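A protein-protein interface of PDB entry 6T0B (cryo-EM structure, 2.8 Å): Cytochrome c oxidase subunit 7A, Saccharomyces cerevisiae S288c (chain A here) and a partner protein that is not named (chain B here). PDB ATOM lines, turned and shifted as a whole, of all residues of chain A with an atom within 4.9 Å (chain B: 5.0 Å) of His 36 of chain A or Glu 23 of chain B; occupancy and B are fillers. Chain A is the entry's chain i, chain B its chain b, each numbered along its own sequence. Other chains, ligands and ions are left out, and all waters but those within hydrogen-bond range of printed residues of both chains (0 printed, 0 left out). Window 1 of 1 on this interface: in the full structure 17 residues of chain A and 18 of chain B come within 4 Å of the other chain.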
ATOM      1  N   TRP A  31     -25.789  18.648  16.938  1.00  0.00           N
ATOM      2  CA  TRP A  31     -25.395  18.712  15.534  1.00  0.00           C
ATOM      3  C   TRP A  31     -24.579  17.500  15.144  1.00  0.00           C
ATOM      4  O   TRP A  31     -25.009  16.710  14.302  1.00  0.00           O
ATOM      5  CB  TRP A  31     -24.598  19.981  15.260  1.00  0.00           C
ATOM      6  CG  TRP A  31     -23.736  19.900  14.037  1.00  0.00           C
ATOM      7  CD1 TRP A  31     -22.398  19.677  13.993  1.00  0.00           C
ATOM      8  CD2 TRP A  31     -24.157  20.059  12.684  1.00  0.00           C
ATOM      9  NE1 TRP A  31     -21.963  19.670  12.698  1.00  0.00           N
ATOM     10  CE2 TRP A  31     -23.027  19.908  11.876  1.00  0.00           C
ATOM     11  CE3 TRP A  31     -25.385  20.312  12.078  1.00  0.00           C
ATOM     12  CZ2 TRP A  31     -23.087  19.998  10.502  1.00  0.00           C
ATOM     13  CZ3 TRP A  31     -25.440  20.403  10.721  1.00  0.00           C
ATOM     14  CH2 TRP A  31     -24.305  20.247   9.945  1.00  0.00           C
ATOM     15  N   TRP A  32     -23.480  17.272  15.859  1.00  0.00           N
ATOM     16  CA  TRP A  32     -22.603  16.136  15.616  1.00  0.00           C
ATOM     17  C   TRP A  32     -23.321  14.811  15.827  1.00  0.00           C
ATOM     18  O   TRP A  32     -23.718  14.182  14.840  1.00  0.00           O
ATOM     19  CB  TRP A  32     -21.382  16.222  16.518  1.00  0.00           C
ATOM     20  CG  TRP A  32     -20.281  15.312  16.138  1.00  0.00           C
ATOM     21  CD1 TRP A  32     -19.944  14.150  16.742  1.00  0.00           C
ATOM     22  CD2 TRP A  32     -19.344  15.501  15.082  1.00  0.00           C
ATOM     23  NE1 TRP A  32     -18.863  13.590  16.123  1.00  0.00           N
ATOM     24  CE2 TRP A  32     -18.474  14.408  15.099  1.00  0.00           C
ATOM     25  CE3 TRP A  32     -19.161  16.490  14.120  1.00  0.00           C
ATOM     26  CZ2 TRP A  32     -17.441  14.270  14.188  1.00  0.00           C
ATOM     27  CZ3 TRP A  32     -18.136  16.351  13.221  1.00  0.00           C
ATOM     28  CH2 TRP A  32     -17.290  15.250  13.260  1.00  0.00           C
ATOM     29  N   GLY A  34     -26.291  13.848  16.344  1.00  0.00           N
ATOM     30  CA  GLY A  34     -27.636  13.564  15.913  1.00  0.00           C
ATOM     31  C   GLY A  34     -27.903  13.831  14.453  1.00  0.00           C
ATOM     32  O   GLY A  34     -28.786  13.195  13.875  1.00  0.00           O
ATOM     33  N   PHE A  35     -27.181  14.757  13.827  1.00  0.00           N
ATOM     34  CA  PHE A  35     -27.276  14.942  12.395  1.00  0.00           C
ATOM     35  C   PHE A  35     -26.094  14.344  11.673  1.00  0.00           C
ATOM     36  O   PHE A  35     -26.281  13.580  10.721  1.00  0.00           O
ATOM     37  CB  PHE A  35     -27.371  16.429  12.062  1.00  0.00           C
ATOM     38  CG  PHE A  35     -27.709  16.706  10.636  1.00  0.00           C
ATOM     39  CD1 PHE A  35     -28.959  16.402  10.139  1.00  0.00           C
ATOM     40  CD2 PHE A  35     -26.782  17.274   9.790  1.00  0.00           C
ATOM     41  CE1 PHE A  35     -29.274  16.658   8.815  1.00  0.00           C
ATOM     42  CE2 PHE A  35     -27.094  17.529   8.471  1.00  0.00           C
ATOM     43  CZ  PHE A  35     -28.341  17.223   7.986  1.00  0.00           C
ATOM     44  N   HIS A  36     -24.883  14.651  12.134  1.00  0.00           N
ATOM     45  CA  HIS A  36     -23.706  14.189  11.431  1.00  0.00           C
ATOM     46  C   HIS A  36     -23.536  12.690  11.599  1.00  0.00           C
ATOM     47  O   HIS A  36     -23.276  11.977  10.627  1.00  0.00           O
ATOM     48  CB  HIS A  36     -22.484  14.936  11.934  1.00  0.00           C
ATOM     49  CG  HIS A  36     -21.198  14.389  11.420  1.00  0.00           C
ATOM     50  ND1 HIS A  36     -20.856  14.425  10.090  1.00  0.00           N
ATOM     51  CD2 HIS A  36     -20.171  13.786  12.057  1.00  0.00           C
ATOM     52  CE1 HIS A  36     -19.672  13.870   9.928  1.00  0.00           C
ATOM     53  NE2 HIS A  36     -19.234  13.473  11.108  1.00  0.00           N
ATOM     54  N   MET A  37     -23.740  12.183  12.807  1.00  0.00           N
ATOM     55  CA  MET A  37     -23.600  10.754  13.014  1.00  0.00           C
ATOM     56  C   MET A  37     -24.877   9.985  12.727  1.00  0.00           C
ATOM     57  O   MET A  37     -24.982   8.820  13.118  1.00  0.00           O
ATOM     58  CB  MET A  37     -23.116  10.474  14.427  1.00  0.00           C
ATOM     59  CG  MET A  37     -21.733  11.002  14.684  1.00  0.00           C
ATOM     60  SD  MET A  37     -20.475  10.113  13.773  1.00  0.00           S
ATOM     61  CE  MET A  37     -20.867   8.432  14.236  1.00  0.00           C
ATOM     62  N   ASP A  38     -25.848  10.605  12.068  1.00  0.00           N
ATOM     63  CA  ASP A  38     -26.895   9.889  11.357  1.00  0.00           C
ATOM     64  C   ASP A  38     -26.581   9.822   9.875  1.00  0.00           C
ATOM     65  O   ASP A  38     -26.792   8.782   9.246  1.00  0.00           O
ATOM     66  CB  ASP A  38     -28.253  10.574  11.585  1.00  0.00           C
ATOM     67  CG  ASP A  38     -29.465   9.731  11.134  1.00  0.00           C
ATOM     68  OD1 ASP A  38     -30.558   9.977  11.681  1.00  0.00           O
ATOM     69  OD2 ASP A  38     -29.380   8.850  10.259  1.00  0.00           O
ATOM     70  N   LYS A  39     -26.096  10.926   9.308  1.00  0.00           N
ATOM     71  CA  LYS A  39     -25.696  10.928   7.911  1.00  0.00           C
ATOM     72  C   LYS A  39     -24.557   9.954   7.673  1.00  0.00           C
ATOM     73  O   LYS A  39     -24.553   9.229   6.670  1.00  0.00           O
ATOM     74  CB  LYS A  39     -25.297  12.338   7.495  1.00  0.00           C
ATOM     75  CG  LYS A  39     -26.454  13.306   7.462  1.00  0.00           C
ATOM     76  CD  LYS A  39     -27.253  13.168   6.179  1.00  0.00           C
ATOM     77  CE  LYS A  39     -28.465  14.084   6.161  1.00  0.00           C
ATOM     78  NZ  LYS A  39     -29.040  14.210   4.800  1.00  0.00           N
ATOM     79  N   ILE A  40     -23.628   9.864   8.627  1.00  0.00           N
ATOM     80  CA  ILE A  40     -22.510   8.937   8.510  1.00  0.00           C
ATOM     81  C   ILE A  40     -22.992   7.495   8.576  1.00  0.00           C
ATOM     82  O   ILE A  40     -22.541   6.643   7.803  1.00  0.00           O
ATOM     83  CB  ILE A  40     -21.465   9.242   9.592  1.00  0.00           C
ATOM     84  CG1 ILE A  40     -20.753  10.545   9.280  1.00  0.00           C
ATOM     85  CG2 ILE A  40     -20.434   8.154   9.701  1.00  0.00           C
ATOM     86  CD1 ILE A  40     -20.097  10.568   7.958  1.00  0.00           C
ATOM     87  N   TYR B   9     -28.366  20.438   2.588  1.00  0.00           N
ATOM     88  CA  TYR B   9     -27.113  19.788   2.901  1.00  0.00           C
ATOM     89  C   TYR B   9     -26.388  19.496   1.597  1.00  0.00           C
ATOM     90  O   TYR B   9     -26.867  19.829   0.512  1.00  0.00           O
ATOM     91  CB  TYR B   9     -27.357  18.514   3.714  1.00  0.00           C
ATOM     92  CG  TYR B   9     -26.173  18.030   4.501  1.00  0.00           C
ATOM     93  CD1 TYR B   9     -25.459  18.890   5.302  1.00  0.00           C
ATOM     94  CD2 TYR B   9     -25.757  16.719   4.416  1.00  0.00           C
ATOM     95  CE1 TYR B   9     -24.381  18.457   6.006  1.00  0.00           C
ATOM     96  CE2 TYR B   9     -24.680  16.278   5.114  1.00  0.00           C
ATOM     97  CZ  TYR B   9     -23.996  17.150   5.909  1.00  0.00           C
ATOM     98  OH  TYR B   9     -22.913  16.709   6.618  1.00  0.00           O
ATOM     99  N   GLU B  19     -16.223  12.838   0.773  1.00  0.00           N
ATOM    100  CA  GLU B  19     -16.591  12.348   2.087  1.00  0.00           C
ATOM    101  C   GLU B  19     -15.650  12.853   3.167  1.00  0.00           C
ATOM    102  O   GLU B  19     -16.012  12.825   4.345  1.00  0.00           O
ATOM    103  CB  GLU B  19     -16.657  10.826   2.083  1.00  0.00           C
ATOM    104  CG  GLU B  19     -15.399  10.120   2.491  1.00  0.00           C
ATOM    105  CD  GLU B  19     -15.514   8.631   2.315  1.00  0.00           C
ATOM    106  OE1 GLU B  19     -16.650   8.142   2.188  1.00  0.00           O
ATOM    107  OE2 GLU B  19     -14.471   7.951   2.291  1.00  0.00           O
ATOM    108  N   GLY B  20     -14.469  13.334   2.803  1.00  0.00           N
ATOM    109  CA  GLY B  20     -13.632  14.008   3.769  1.00  0.00           C
ATOM    110  C   GLY B  20     -14.022  15.460   3.915  1.00  0.00           C
ATOM    111  O   GLY B  20     -13.903  16.033   4.999  1.00  0.00           O
ATOM    112  N   ILE B  21     -14.449  16.064   2.810  1.00  0.00           N
ATOM    113  CA  ILE B  21     -14.886  17.455   2.809  1.00  0.00           C
ATOM    114  C   ILE B  21     -16.111  17.615   3.687  1.00  0.00           C
ATOM    115  O   ILE B  21     -16.227  18.580   4.451  1.00  0.00           O
ATOM    116  CB  ILE B  21     -15.151  17.913   1.363  1.00  0.00           C
ATOM    117  CG1 ILE B  21     -13.852  18.249   0.657  1.00  0.00           C
ATOM    118  CG2 ILE B  21     -16.046  19.120   1.297  1.00  0.00           C
ATOM    119  CD1 ILE B  21     -13.971  18.160  -0.814  1.00  0.00           C
ATOM    120  N   LEU B  22     -17.008  16.628   3.641  1.00  0.00           N
ATOM    121  CA  LEU B  22     -18.192  16.636   4.492  1.00  0.00           C
ATOM    122  C   LEU B  22     -17.823  16.534   5.966  1.00  0.00           C
ATOM    123  O   LEU B  22     -18.405  17.232   6.805  1.00  0.00           O
ATOM    124  CB  LEU B  22     -19.108  15.491   4.080  1.00  0.00           C
ATOM    125  CG  LEU B  22     -20.523  15.352   4.616  1.00  0.00           C
ATOM    126  CD1 LEU B  22     -21.384  14.833   3.503  1.00  0.00           C
ATOM    127  CD2 LEU B  22     -20.578  14.394   5.794  1.00  0.00           C
ATOM    128  N   GLU B  23     -16.828  15.712   6.298  1.00  0.00           N
ATOM    129  CA  GLU B  23     -16.454  15.550   7.699  1.00  0.00           C
ATOM    130  C   GLU B  23     -15.726  16.774   8.230  1.00  0.00           C
ATOM    131  O   GLU B  23     -15.939  17.174   9.378  1.00  0.00           O
ATOM    132  CB  GLU B  23     -15.596  14.306   7.887  1.00  0.00           C
ATOM    133  CG  GLU B  23     -15.397  13.948   9.344  1.00  0.00           C
ATOM    134  CD  GLU B  23     -15.157  12.479   9.555  1.00  0.00           C
ATOM    135  OE1 GLU B  23     -14.204  11.942   8.957  1.00  0.00           O
ATOM    136  OE2 GLU B  23     -15.924  11.857  10.314  1.00  0.00           O
ATOM    137  N   LEU B  24     -14.877  17.387   7.410  1.00  0.00           N
ATOM    138  CA  LEU B  24     -14.224  18.622   7.818  1.00  0.00           C
ATOM    139  C   LEU B  24     -15.229  19.749   7.983  1.00  0.00           C
ATOM    140  O   LEU B  24     -15.121  20.546   8.920  1.00  0.00           O
ATOM    141  CB  LEU B  24     -13.161  19.012   6.803  1.00  0.00           C
ATOM    142  CG  LEU B  24     -12.554  20.399   6.935  1.00  0.00           C
ATOM    143  CD1 LEU B  24     -11.637  20.435   8.124  1.00  0.00           C
ATOM    144  CD2 LEU B  24     -11.824  20.762   5.680  1.00  0.00           C
ATOM    145  N   HIS B  25     -16.226  19.811   7.099  1.00  0.00           N
ATOM    146  CA  HIS B  25     -17.260  20.826   7.215  1.00  0.00           C
ATOM    147  C   HIS B  25     -18.069  20.642   8.480  1.00  0.00           C
ATOM    148  O   HIS B  25     -18.389  21.618   9.164  1.00  0.00           O
ATOM    149  CB  HIS B  25     -18.188  20.786   6.014  1.00  0.00           C
ATOM    150  CG  HIS B  25     -19.394  21.650   6.176  1.00  0.00           C
ATOM    151  ND1 HIS B  25     -20.608  21.162   6.601  1.00  0.00           N
ATOM    152  CD2 HIS B  25     -19.564  22.979   6.002  1.00  0.00           C
ATOM    153  CE1 HIS B  25     -21.478  22.150   6.665  1.00  0.00           C
ATOM    154  NE2 HIS B  25     -20.870  23.264   6.308  1.00  0.00           N
ATOM    155  N   ASP B  26     -18.383  19.396   8.826  1.00  0.00           N
ATOM    156  CA  ASP B  26     -19.143  19.170  10.042  1.00  0.00           C
ATOM    157  C   ASP B  26     -18.308  19.429  11.283  1.00  0.00           C
ATOM    158  O   ASP B  26     -18.829  19.932  12.285  1.00  0.00           O
ATOM    159  CB  ASP B  26     -19.699  17.760  10.042  1.00  0.00           C
ATOM    160  CG  ASP B  26     -20.769  17.581   9.014  1.00  0.00           C
ATOM    161  OD1 ASP B  26     -21.098  18.573   8.347  1.00  0.00           O
ATOM    162  OD2 ASP B  26     -21.288  16.460   8.874  1.00  0.00           O
ATOM    163  N   ASN B  27     -17.011  19.133  11.224  1.00  0.00           N
ATOM    164  CA  ASN B  27     -16.130  19.399  12.353  1.00  0.00           C
ATOM    165  C   ASN B  27     -15.958  20.891  12.579  1.00  0.00           C
ATOM    166  O   ASN B  27     -15.866  21.343  13.719  1.00  0.00           O
ATOM    167  CB  ASN B  27     -14.781  18.735  12.114  1.00  0.00           C
ATOM    168  CG  ASN B  27     -14.098  18.355  13.381  1.00  0.00           C
ATOM    169  OD1 ASN B  27     -14.189  19.060  14.381  1.00  0.00           O
ATOM    170  ND2 ASN B  27     -13.403  17.230  13.362  1.00  0.00           N
ATOM    171  N   ILE B  28     -15.900  21.667  11.502  1.00  0.00           N
ATOM    172  CA  ILE B  28     -15.844  23.116  11.624  1.00  0.00           C
ATOM    173  C   ILE B  28     -17.162  23.649  12.154  1.00  0.00           C
ATOM    174  O   ILE B  28     -17.186  24.498  13.053  1.00  0.00           O
ATOM    175  CB  ILE B  28     -15.483  23.736  10.264  1.00  0.00           C
ATOM    176  CG1 ILE B  28     -14.037  23.443   9.911  1.00  0.00           C
ATOM    177  CG2 ILE B  28     -15.673  25.214  10.272  1.00  0.00           C
ATOM    178  CD1 ILE B  28     -13.676  23.862   8.531  1.00  0.00           C
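O of Asp 26 of chain B is in hydrogen-bond range of NE1 of Trp 31 of chain A (3.2 Å).
OD2 of Asp 26 of chain B lies within hydrogen-bond range of ND1 of His 36 of chain A, 2.4 Å away.
OD2 of Asp 26 of chain B is in hydrogen-bond range of OH of Tyr 9 of chain B (2.8 Å).
A ring nitrogen (ND1) of His 25 of chain B is in hydrogen-bond range of the side-chain carboxylate (OD1) of Asp 26 of chain B, 3.2 Å away.
The backbone NH of His 36 of chain A sits at hydrogen-bond distance from the backbone carbonyl oxygen of Trp 31 of chain A (3.0 Å).
O of Trp 32 of chain A sits at hydrogen-bond distance from N of Met 37 of chain A (2.9 Å).
Trp 32 of chain A touches Asp 26 of chain B (CZ3 to C, 3.6 Å).
Asn 27 of chain B touches Trp 32 of chain A (N to CZ3, 3.6 Å).
Tyr 9 of chain B touches Phe 35 of chain A (CE1 to CE2, 3.8 Å).
OE2 of Glu 23 of chain B touches NE2 of His 36 of chain A (3.8 Å).
His 36 of chain A touches just these residues of chain B: Glu 23 and Asp 26.
Of the printed residues of chain A, Glu 23 of chain B touches His 36 (3.8 Å).
Printed residues of chain B within 4 Å of Trp 32 of chain A: Asp 26 (3.6 Å) and Asn 27 (3.6 Å).
Of the printed residues of chain B, Phe 35 of chain A touches Tyr 9 (3.8 Å).
Of the printed residues of chain A, Asn 27 of chain B touches Trp 32.
Gly 20 of chain B touches none of the printed residues of chain A.
The nearest residue of chain A that does not touch Glu 23 of chain B is Trp 32 of chain A (4.5 Å).
The nearest printed residue of chain B that does not touch Trp 32 of chain A is Glu 23 of chain B (4.5 Å).
Among the printed residues, 6 pairs touch across the chains.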
